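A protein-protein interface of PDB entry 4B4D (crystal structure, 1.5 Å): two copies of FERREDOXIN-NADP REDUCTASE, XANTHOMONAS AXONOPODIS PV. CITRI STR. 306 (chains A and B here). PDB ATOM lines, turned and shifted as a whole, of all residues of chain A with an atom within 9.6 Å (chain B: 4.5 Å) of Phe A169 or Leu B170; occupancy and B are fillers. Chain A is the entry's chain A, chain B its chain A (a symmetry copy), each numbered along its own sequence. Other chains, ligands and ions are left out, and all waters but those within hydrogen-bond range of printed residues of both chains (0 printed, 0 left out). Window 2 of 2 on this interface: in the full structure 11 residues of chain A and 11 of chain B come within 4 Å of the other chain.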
ATOM      1  N   TRP A  64     -23.358  -9.827  16.837  1.00  0.00           N
ATOM      2  CA  TRP A  64     -24.675  -9.485  16.289  1.00  0.00           C
ATOM      3  C   TRP A  64     -24.682  -9.487  14.781  1.00  0.00           C
ATOM      4  O   TRP A  64     -25.756  -9.525  14.167  1.00  0.00           O
ATOM      5  CB  TRP A  64     -25.193  -8.152  16.857  1.00  0.00           C
ATOM      6  CG  TRP A  64     -24.358  -6.952  16.491  1.00  0.00           C
ATOM      7  CD1 TRP A  64     -23.408  -6.311  17.282  1.00  0.00           C
ATOM      8  CD2 TRP A  64     -24.347  -6.222  15.218  1.00  0.00           C
ATOM      9  NE1 TRP A  64     -22.840  -5.261  16.608  1.00  0.00           N
ATOM     10  CE2 TRP A  64     -23.355  -5.154  15.365  1.00  0.00           C
ATOM     11  CE3 TRP A  64     -25.040  -6.340  14.013  1.00  0.00           C
ATOM     12  CZ2 TRP A  64     -23.079  -4.259  14.341  1.00  0.00           C
ATOM     13  CZ3 TRP A  64     -24.758  -5.434  12.988  1.00  0.00           C
ATOM     14  CH2 TRP A  64     -23.800  -4.414  13.150  1.00  0.00           C
ATOM     15  N   ILE A 130     -15.150  -2.795  19.151  1.00  0.00           N
ATOM     16  CA  ILE A 130     -15.673  -1.460  18.843  1.00  0.00           C
ATOM     17  C   ILE A 130     -17.087  -1.481  18.247  1.00  0.00           C
ATOM     18  O   ILE A 130     -17.739  -0.442  18.167  1.00  0.00           O
ATOM     19  CB  ILE A 130     -14.717  -0.649  17.938  1.00  0.00           C
ATOM     20  CG1 ILE A 130     -14.628  -1.252  16.525  1.00  0.00           C
ATOM     21  CG2 ILE A 130     -13.341  -0.537  18.593  1.00  0.00           C
ATOM     22  CD1 ILE A 130     -13.634  -0.549  15.617  1.00  0.00           C
ATOM     23  N   LYS A 131     -17.544  -2.660  17.835  1.00  0.00           N
ATOM     24  CA  LYS A 131     -18.920  -2.816  17.318  1.00  0.00           C
ATOM     25  C   LYS A 131     -19.900  -3.427  18.331  1.00  0.00           C
ATOM     26  O   LYS A 131     -21.081  -3.655  18.016  1.00  0.00           O
ATOM     27  CB  LYS A 131     -18.905  -3.581  15.981  1.00  0.00           C
ATOM     28  CG  LYS A 131     -18.315  -2.771  14.836  1.00  0.00           C
ATOM     29  CD  LYS A 131     -18.600  -3.397  13.478  1.00  0.00           C
ATOM     30  CE  LYS A 131     -17.587  -4.476  13.126  1.00  0.00           C
ATOM     31  NZ  LYS A 131     -17.688  -4.879  11.693  1.00  0.00           N
ATOM     32  N   PRO A 133     -22.292  -2.947  21.335  1.00  0.00           N
ATOM     33  CA  PRO A 133     -22.960  -1.844  22.046  1.00  0.00           C
ATOM     34  C   PRO A 133     -22.591  -1.754  23.528  1.00  0.00           C
ATOM     35  O   PRO A 133     -22.562  -0.654  24.090  1.00  0.00           O
ATOM     36  CB  PRO A 133     -24.457  -2.179  21.888  1.00  0.00           C
ATOM     37  CG  PRO A 133     -24.501  -3.648  21.594  1.00  0.00           C
ATOM     38  CD  PRO A 133     -23.254  -3.940  20.805  1.00  0.00           C
ATOM     39  N   TYR A 136     -19.739   0.586  24.785  1.00  0.00           N
ATOM     40  CA  TYR A 136     -20.061   1.991  25.000  1.00  0.00           C
ATOM     41  C   TYR A 136     -20.954   2.234  26.207  1.00  0.00           C
ATOM     42  O   TYR A 136     -20.932   3.315  26.774  1.00  0.00           O
ATOM     43  CB  TYR A 136     -20.627   2.607  23.720  1.00  0.00           C
ATOM     44  CG  TYR A 136     -19.663   2.406  22.571  1.00  0.00           C
ATOM     45  CD1 TYR A 136     -18.522   3.211  22.440  1.00  0.00           C
ATOM     46  CD2 TYR A 136     -19.829   1.348  21.677  1.00  0.00           C
ATOM     47  CE1 TYR A 136     -17.614   3.001  21.409  1.00  0.00           C
ATOM     48  CE2 TYR A 136     -18.928   1.133  20.647  1.00  0.00           C
ATOM     49  CZ  TYR A 136     -17.817   1.959  20.521  1.00  0.00           C
ATOM     50  OH  TYR A 136     -16.931   1.738  19.507  1.00  0.00           O
ATOM     51  N   GLU A 163     -15.783   6.104   7.656  1.00  0.00           N
ATOM     52  CA  GLU A 163     -17.010   5.314   7.503  1.00  0.00           C
ATOM     53  C   GLU A 163     -17.716   5.021   8.822  1.00  0.00           C
ATOM     54  O   GLU A 163     -18.933   5.187   8.937  1.00  0.00           O
ATOM     55  CB  GLU A 163     -16.727   4.010   6.756  1.00  0.00           C
ATOM     56  CG  GLU A 163     -16.140   4.191   5.364  1.00  0.00           C
ATOM     57  CD  GLU A 163     -15.540   2.908   4.812  1.00  0.00           C
ATOM     58  OE1 GLU A 163     -15.893   1.815   5.306  1.00  0.00           O
ATOM     59  OE2 GLU A 163     -14.709   2.994   3.879  1.00  0.00           O
ATOM     60  N   LEU A 164     -16.947   4.583   9.813  1.00  0.00           N
ATOM     61  CA  LEU A 164     -17.494   4.182  11.105  1.00  0.00           C
ATOM     62  C   LEU A 164     -18.213   5.323  11.848  1.00  0.00           C
ATOM     63  O   LEU A 164     -19.254   5.078  12.466  1.00  0.00           O
ATOM     64  CB  LEU A 164     -16.403   3.530  11.966  1.00  0.00           C
ATOM     65  CG  LEU A 164     -16.780   2.541  13.065  1.00  0.00           C
ATOM     66  CD1 LEU A 164     -17.800   1.499  12.617  1.00  0.00           C
ATOM     67  CD2 LEU A 164     -15.525   1.865  13.590  1.00  0.00           C
ATOM     68  N   PRO A 165     -17.684   6.568  11.777  1.00  0.00           N
ATOM     69  CA  PRO A 165     -18.441   7.705  12.332  1.00  0.00           C
ATOM     70  C   PRO A 165     -19.783   7.986  11.631  1.00  0.00           C
ATOM     71  O   PRO A 165     -20.545   8.837  12.094  1.00  0.00           O
ATOM     72  CB  PRO A 165     -17.492   8.891  12.128  1.00  0.00           C
ATOM     73  CG  PRO A 165     -16.136   8.283  12.086  1.00  0.00           C
ATOM     74  CD  PRO A 165     -16.319   6.975  11.383  1.00  0.00           C
ATOM     75  N   GLN A 166     -20.048   7.283  10.530  1.00  0.00           N
ATOM     76  CA  GLN A 166     -21.313   7.382   9.789  1.00  0.00           C
ATOM     77  C   GLN A 166     -22.171   6.122   9.883  1.00  0.00           C
ATOM     78  O   GLN A 166     -23.193   6.023   9.204  1.00  0.00           O
ATOM     79  CB  GLN A 166     -21.044   7.685   8.309  1.00  0.00           C
ATOM     80  CG  GLN A 166     -21.221   9.136   7.907  1.00  0.00           C
ATOM     81  CD  GLN A 166     -20.066  10.012   8.339  1.00  0.00           C
ATOM     82  OE1 GLN A 166     -19.926  10.342   9.516  1.00  0.00           O
ATOM     83  NE2 GLN A 166     -19.237  10.405   7.382  1.00  0.00           N
ATOM     84  N   HIS A 167     -21.755   5.163  10.709  1.00  0.00           N
ATOM     85  CA  HIS A 167     -22.482   3.902  10.883  1.00  0.00           C
ATOM     86  C   HIS A 167     -23.920   4.197  11.198  1.00  0.00           C
ATOM     87  O   HIS A 167     -24.245   4.619  12.311  1.00  0.00           O
ATOM     88  CB  HIS A 167     -21.854   3.073  12.001  1.00  0.00           C
ATOM     89  CG  HIS A 167     -22.254   1.613  11.990  1.00  0.00           C
ATOM     90  ND1 HIS A 167     -23.502   1.198  12.281  1.00  0.00           N
ATOM     91  CD2 HIS A 167     -21.506   0.463  11.732  1.00  0.00           C
ATOM     92  CE1 HIS A 167     -23.559  -0.147  12.198  1.00  0.00           C
ATOM     93  NE2 HIS A 167     -22.336  -0.597  11.865  1.00  0.00           N
ATOM     94  N   GLU A 168     -24.791   4.000  10.208  1.00  0.00           N
ATOM     95  CA  GLU A 168     -26.228   4.284  10.334  1.00  0.00           C
ATOM     96  C   GLU A 168     -26.782   4.037  11.752  1.00  0.00           C
ATOM     97  O   GLU A 168     -27.736   4.695  12.175  1.00  0.00           O
ATOM     98  CB  GLU A 168     -27.016   3.486   9.279  1.00  0.00           C
ATOM     99  CG  GLU A 168     -28.516   3.769   9.201  1.00  0.00           C
ATOM    100  CD  GLU A 168     -28.850   5.172   8.719  1.00  0.00           C
ATOM    101  OE1 GLU A 168     -28.299   5.621   7.690  1.00  0.00           O
ATOM    102  OE2 GLU A 168     -29.690   5.829   9.365  1.00  0.00           O
ATOM    103  N   PHE A 169     -26.158   3.118  12.488  1.00  0.00           N
ATOM    104  CA  PHE A 169     -26.627   2.740  13.818  1.00  0.00           C
ATOM    105  C   PHE A 169     -25.690   3.020  14.993  1.00  0.00           C
ATOM    106  O   PHE A 169     -26.155   3.311  16.098  1.00  0.00           O
ATOM    107  CB  PHE A 169     -26.981   1.269  13.823  1.00  0.00           C
ATOM    108  CG  PHE A 169     -28.145   0.930  12.951  1.00  0.00           C
ATOM    109  CD1 PHE A 169     -29.385   1.523  13.163  1.00  0.00           C
ATOM    110  CD2 PHE A 169     -28.004   0.016  11.918  1.00  0.00           C
ATOM    111  CE1 PHE A 169     -30.464   1.200  12.363  1.00  0.00           C
ATOM    112  CE2 PHE A 169     -29.082  -0.311  11.115  1.00  0.00           C
ATOM    113  CZ  PHE A 169     -30.311   0.285  11.333  1.00  0.00           C
ATOM    114  N   LEU A 170     -24.383   2.898  14.774  1.00  0.00           N
ATOM    115  CA  LEU A 170     -23.414   3.119  15.847  1.00  0.00           C
ATOM    116  C   LEU A 170     -22.797   4.517  15.793  1.00  0.00           C
ATOM    117  O   LEU A 170     -22.214   4.976  16.776  1.00  0.00           O
ATOM    118  CB  LEU A 170     -22.317   2.047  15.814  1.00  0.00           C
ATOM    119  CG  LEU A 170     -22.658   0.618  16.254  1.00  0.00           C
ATOM    120  CD1 LEU A 170     -21.611  -0.361  15.736  1.00  0.00           C
ATOM    121  CD2 LEU A 170     -22.810   0.495  17.765  1.00  0.00           C
ATOM    122  N   GLY A 171     -22.963   5.188  14.654  1.00  0.00           N
ATOM    123  CA  GLY A 171     -22.296   6.459  14.333  1.00  0.00           C
ATOM    124  C   GLY A 171     -22.318   7.608  15.331  1.00  0.00           C
ATOM    125  O   GLY A 171     -21.271   8.197  15.616  1.00  0.00           O
ATOM    126  N   ASP A 172     -23.501   7.944  15.843  1.00  0.00           N
ATOM    127  CA  ASP A 172     -23.657   9.068  16.780  1.00  0.00           C
ATOM    128  C   ASP A 172     -22.812   8.858  18.034  1.00  0.00           C
ATOM    129  O   ASP A 172     -22.117   9.766  18.504  1.00  0.00           O
ATOM    130  CB  ASP A 172     -25.133   9.244  17.174  1.00  0.00           C
ATOM    131  CG  ASP A 172     -26.031   9.540  15.982  1.00  0.00           C
ATOM    132  OD1 ASP A 172     -25.517   9.962  14.927  1.00  0.00           O
ATOM    133  OD2 ASP A 172     -27.261   9.351  16.102  1.00  0.00           O
ATOM    134  N   LEU A 173     -22.890   7.640  18.553  1.00  0.00           N
ATOM    135  CA  LEU A 173     -22.129   7.197  19.707  1.00  0.00           C
ATOM    136  C   LEU A 173     -20.620   7.188  19.446  1.00  0.00           C
ATOM    137  O   LEU A 173     -19.830   7.556  20.319  1.00  0.00           O
ATOM    138  CB  LEU A 173     -22.600   5.793  20.067  1.00  0.00           C
ATOM    139  CG  LEU A 173     -22.277   5.155  21.407  1.00  0.00           C
ATOM    140  CD1 LEU A 173     -22.611   6.062  22.586  1.00  0.00           C
ATOM    141  CD2 LEU A 173     -23.081   3.866  21.471  1.00  0.00           C
ATOM    142  N   LEU A 174     -20.231   6.772  18.243  1.00  0.00           N
ATOM    143  CA  LEU A 174     -18.820   6.627  17.889  1.00  0.00           C
ATOM    144  C   LEU A 174     -18.110   7.961  17.745  1.00  0.00           C
ATOM    145  O   LEU A 174     -16.959   8.094  18.161  1.00  0.00           O
ATOM    146  CB  LEU A 174     -18.650   5.790  16.616  1.00  0.00           C
ATOM    147  CG  LEU A 174     -19.271   4.391  16.681  1.00  0.00           C
ATOM    148  CD1 LEU A 174     -18.945   3.584  15.440  1.00  0.00           C
ATOM    149  CD2 LEU A 174     -18.831   3.632  17.914  1.00  0.00           C
ATOM    150  N   ARG A 175     -18.789   8.952  17.168  1.00  0.00           N
ATOM    151  CA  ARG A 175     -18.220  10.296  17.079  1.00  0.00           C
ATOM    152  C   ARG A 175     -17.923  10.843  18.474  1.00  0.00           C
ATOM    153  O   ARG A 175     -16.963  11.579  18.663  1.00  0.00           O
ATOM    154  CB  ARG A 175     -19.143  11.238  16.294  1.00  0.00           C
ATOM    155  CG  ARG A 175     -19.102  10.989  14.793  1.00  0.00           C
ATOM    156  CD  ARG A 175     -19.838  12.050  13.979  1.00  0.00           C
ATOM    157  NE  ARG A 175     -21.211  12.273  14.439  1.00  0.00           N
ATOM    158  CZ  ARG A 175     -22.263  11.510  14.138  1.00  0.00           C
ATOM    159  NH1 ARG A 175     -22.140  10.442  13.361  1.00  0.00           N
ATOM    160  NH2 ARG A 175     -23.459  11.820  14.620  1.00  0.00           N
ATOM    161  N   TRP B  64     -28.347   1.947   3.316  1.00  0.00           N
ATOM    162  CA  TRP B  64     -27.289   2.030   4.330  1.00  0.00           C
ATOM    163  C   TRP B  64     -26.497   0.751   4.432  1.00  0.00           C
ATOM    164  O   TRP B  64     -25.398   0.746   5.000  1.00  0.00           O
ATOM    165  CB  TRP B  64     -27.851   2.461   5.697  1.00  0.00           C
ATOM    166  CG  TRP B  64     -28.823   1.484   6.307  1.00  0.00           C
ATOM    167  CD1 TRP B  64     -30.212   1.563   6.304  1.00  0.00           C
ATOM    168  CD2 TRP B  64     -28.514   0.232   7.008  1.00  0.00           C
ATOM    169  NE1 TRP B  64     -30.762   0.484   6.948  1.00  0.00           N
ATOM    170  CE2 TRP B  64     -29.801  -0.353   7.389  1.00  0.00           C
ATOM    171  CE3 TRP B  64     -27.338  -0.438   7.348  1.00  0.00           C
ATOM    172  CZ2 TRP B  64     -29.889  -1.556   8.076  1.00  0.00           C
ATOM    173  CZ3 TRP B  64     -27.435  -1.647   8.041  1.00  0.00           C
ATOM    174  CH2 TRP B  64     -28.684  -2.192   8.399  1.00  0.00           C
ATOM    175  N   LYS B 131     -36.394  -1.570   6.321  1.00  0.00           N
ATOM    176  CA  LYS B 131     -35.075  -1.321   6.939  1.00  0.00           C
ATOM    177  C   LYS B 131     -34.617   0.143   6.862  1.00  0.00           C
ATOM    178  O   LYS B 131     -33.507   0.487   7.304  1.00  0.00           O
ATOM    179  CB  LYS B 131     -34.025  -2.295   6.369  1.00  0.00           C
ATOM    180  CG  LYS B 131     -34.233  -3.731   6.828  1.00  0.00           C
ATOM    181  CD  LYS B 131     -33.026  -4.611   6.534  1.00  0.00           C
ATOM    182  CE  LYS B 131     -33.049  -5.150   5.112  1.00  0.00           C
ATOM    183  NZ  LYS B 131     -32.039  -6.231   4.917  1.00  0.00           N
ATOM    184  N   HIS B 167     -33.412  -7.387  15.647  1.00  0.00           N
ATOM    185  CA  HIS B 167     -32.388  -6.610  14.941  1.00  0.00           C
ATOM    186  C   HIS B 167     -31.672  -5.725  15.920  1.00  0.00           C
ATOM    187  O   HIS B 167     -32.221  -4.718  16.374  1.00  0.00           O
ATOM    188  CB  HIS B 167     -33.022  -5.771  13.834  1.00  0.00           C
ATOM    189  CG  HIS B 167     -32.039  -5.264  12.800  1.00  0.00           C
ATOM    190  ND1 HIS B 167     -31.107  -4.331  13.078  1.00  0.00           N
ATOM    191  CD2 HIS B 167     -31.888  -5.581  11.449  1.00  0.00           C
ATOM    192  CE1 HIS B 167     -30.385  -4.073  11.968  1.00  0.00           C
ATOM    193  NE2 HIS B 167     -30.866  -4.837  10.971  1.00  0.00           N
ATOM    194  N   GLU B 168     -30.445  -6.110  16.272  1.00  0.00           N
ATOM    195  CA  GLU B 168     -29.626  -5.384  17.254  1.00  0.00           C
ATOM    196  C   GLU B 168     -29.854  -3.859  17.238  1.00  0.00           C
ATOM    197  O   GLU B 168     -29.710  -3.194  18.266  1.00  0.00           O
ATOM    198  CB  GLU B 168     -28.138  -5.729  17.055  1.00  0.00           C
ATOM    199  CG  GLU B 168     -27.168  -5.147  18.083  1.00  0.00           C
ATOM    200  CD  GLU B 168     -27.346  -5.712  19.483  1.00  0.00           C
ATOM    201  OE1 GLU B 168     -27.415  -6.950  19.647  1.00  0.00           O
ATOM    202  OE2 GLU B 168     -27.398  -4.910  20.437  1.00  0.00           O
ATOM    203  N   PHE B 169     -30.244  -3.323  16.081  1.00  0.00           N
ATOM    204  CA  PHE B 169     -30.424  -1.884  15.915  1.00  0.00           C
ATOM    205  C   PHE B 169     -31.834  -1.391  15.587  1.00  0.00           C
ATOM    206  O   PHE B 169     -32.217  -0.295  16.003  1.00  0.00           O
ATOM    207  CB  PHE B 169     -29.477  -1.382  14.847  1.00  0.00           C
ATOM    208  CG  PHE B 169     -28.036  -1.495  15.224  1.00  0.00           C
ATOM    209  CD1 PHE B 169     -27.548  -0.859  16.360  1.00  0.00           C
ATOM    210  CD2 PHE B 169     -27.163  -2.237  14.441  1.00  0.00           C
ATOM    211  CE1 PHE B 169     -26.213  -0.954  16.700  1.00  0.00           C
ATOM    212  CE2 PHE B 169     -25.826  -2.335  14.778  1.00  0.00           C
ATOM    213  CZ  PHE B 169     -25.350  -1.698  15.910  1.00  0.00           C
ATOM    214  N   LEU B 170     -32.588  -2.171  14.817  1.00  0.00           N
ATOM    215  CA  LEU B 170     -33.939  -1.768  14.429  1.00  0.00           C
ATOM    216  C   LEU B 170     -35.013  -2.420  15.301  1.00  0.00           C
ATOM    217  O   LEU B 170     -36.157  -1.963  15.322  1.00  0.00           O
ATOM    218  CB  LEU B 170     -34.192  -2.077  12.948  1.00  0.00           C
ATOM    219  CG  LEU B 170     -33.500  -1.220  11.879  1.00  0.00           C
ATOM    220  CD1 LEU B 170     -33.507  -1.939  10.535  1.00  0.00           C
ATOM    221  CD2 LEU B 170     -34.121   0.166  11.753  1.00  0.00           C
ATOM    222  N   GLY B 171     -34.621  -3.461  16.034  1.00  0.00           N
ATOM    223  CA  GLY B 171     -35.530  -4.335  16.790  1.00  0.00           C
ATOM    224  C   GLY B 171     -36.581  -3.733  17.713  1.00  0.00           C
ATOM    225  O   GLY B 171     -37.752  -4.119  17.650  1.00  0.00           O
ATOM    226  N   ASP B 172     -36.167  -2.811  18.581  1.00  0.00           N
ATOM    227  CA  ASP B 172     -37.078  -2.190  19.556  1.00  0.00           C
ATOM    228  C   ASP B 172     -38.232  -1.478  18.854  1.00  0.00           C
ATOM    229  O   ASP B 172     -39.401  -1.611  19.232  1.00  0.00           O
ATOM    230  CB  ASP B 172     -36.321  -1.194  20.448  1.00  0.00           C
ATOM    231  CG  ASP B 172     -35.203  -1.848  21.248  1.00  0.00           C
ATOM    232  OD1 ASP B 172     -35.219  -3.085  21.409  1.00  0.00           O
ATOM    233  OD2 ASP B 172     -34.304  -1.119  21.719  1.00  0.00           O
ATOM    234  N   LEU B 173     -37.868  -0.727  17.823  1.00  0.00           N
ATOM    235  CA  LEU B 173     -38.799  -0.007  16.972  1.00  0.00           C
ATOM    236  C   LEU B 173     -39.729  -0.943  16.196  1.00  0.00           C
ATOM    237  O   LEU B 173     -40.918  -0.658  16.039  1.00  0.00           O
ATOM    238  CB  LEU B 173     -37.985   0.838  15.999  1.00  0.00           C
ATOM    239  CG  LEU B 173     -38.609   1.968  15.198  1.00  0.00           C
ATOM    240  CD1 LEU B 173     -39.417   2.927  16.066  1.00  0.00           C
ATOM    241  CD2 LEU B 173     -37.460   2.693  14.516  1.00  0.00           C
ATOM    242  N   LEU B 174     -39.180  -2.058  15.720  1.00  0.00           N
ATOM    243  CA  LEU B 174     -39.928  -2.997  14.885  1.00  0.00           C
ATOM    244  C   LEU B 174     -40.991  -3.756  15.661  1.00  0.00           C
ATOM    245  O   LEU B 174     -42.086  -3.979  15.147  1.00  0.00           O
ATOM    246  CB  LEU B 174     -38.988  -3.975  14.170  1.00  0.00           C
ATOM    247  CG  LEU B 174     -37.917  -3.311  13.298  1.00  0.00           C
ATOM    248  CD1 LEU B 174     -37.119  -4.341  12.524  1.00  0.00           C
ATOM    249  CD2 LEU B 174     -38.511  -2.300  12.341  1.00  0.00           C
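Printed residues of chain B that touch a printed residue of chain A: Trp B64, Glu B168, Phe B169 and Leu B170.
Hydrophobic or aromatic side chains of chain B that line the printed part of chain A: Trp B64, Phe B169 and Leu B170.
Along chain A the printed residues that touch a printed residue of chain B span positions 64 to 170.
Among the printed residues, no Asp or Glu carboxylate lies within 4 Å of a Lys or Arg side-chain nitrogen of the other chain.
Printed residues of chain B within 4 Å of Trp A64: Glu B168 and Phe B169.
Of the printed residues of chain B, Pro A133 touches Glu B168.
Pro A165 touches none of the printed residues of chain B.
Of the printed residues of chain B, Glu A168 touches Trp B64.
Phe A169 touches just these residues of chain B: Trp B64 (3.3 Å), Phe B169 (3.3 Å) and Leu B170 (3.6 Å).
Printed residues of chain B within 4 Å of Leu A170: Phe B169 (3.6 Å).
Printed residues of chain A within 4 Å of Trp B64: Glu A168 (3.7 Å) and Phe A169 (3.3 Å).
Of chain A, only Trp A64 (3.3 Å), Phe A169 (3.3 Å) and Leu A170 (3.6 Å) come within 4 Å of Phe B169.
Printed residues of chain A within 4 Å of Leu B170: Phe A169.
No residue of chain A comes within 4 Å of Gly B171.
Leu B174 touches none of the printed residues of chain A.
The nearest residue of chain B that does not touch Phe A169 is His B167 (4.1 Å).
Among the printed residues, merely in contact across the chains: Phe A169 with Phe B169, Phe A169 with Trp B64, Trp A64 with Phe B169, Pro A133 with Glu B168, Leu A170 with Phe B169, Phe A169 with Leu B170, Trp A64 with Glu B168 and Glu A168 with Trp B64.
The backbone carbonyl oxygen (O) of Lys A131 sits at hydrogen-bond distance from the indole nitrogen (NE1) of Trp A64, 2.8 Å away.
N of Phe A169 lies close to ND1 of His A167.
A ring nitrogen (ND1) of His A167 lies within hydrogen-bond range of the backbone NH of Leu A170 (3.1 Å).
The indole nitrogen of Trp B64 sits at hydrogen-bond distance from the backbone carbonyl oxygen of Lys B131 (2.8 Å).
ND1 of His B167 lies close to N of Phe B169.
A ring nitrogen (ND1) of His B167 lies within hydrogen-bond range of the backbone NH (N) of Leu B170 (3.1 Å).
Trp A64 touches Glu B168, and with the chains exchanged Glu A168 touches Trp B64.
Trp A64 touches Phe B169, and with the chains exchanged Phe A169 touches Trp B64.
Phe A169 touches its own counterpart, Phe B169.
Phe A169 touches Leu B170, and with the chains exchanged Leu A170 touches Phe B169.
Positions printed for both chains: 64, 131, 167, 168, 169, 170, 171, 172, 173 and 174.
Of the 8 pairs that touch across the chains among the printed residues, 7 have their exchanged pair printed and touching as well.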
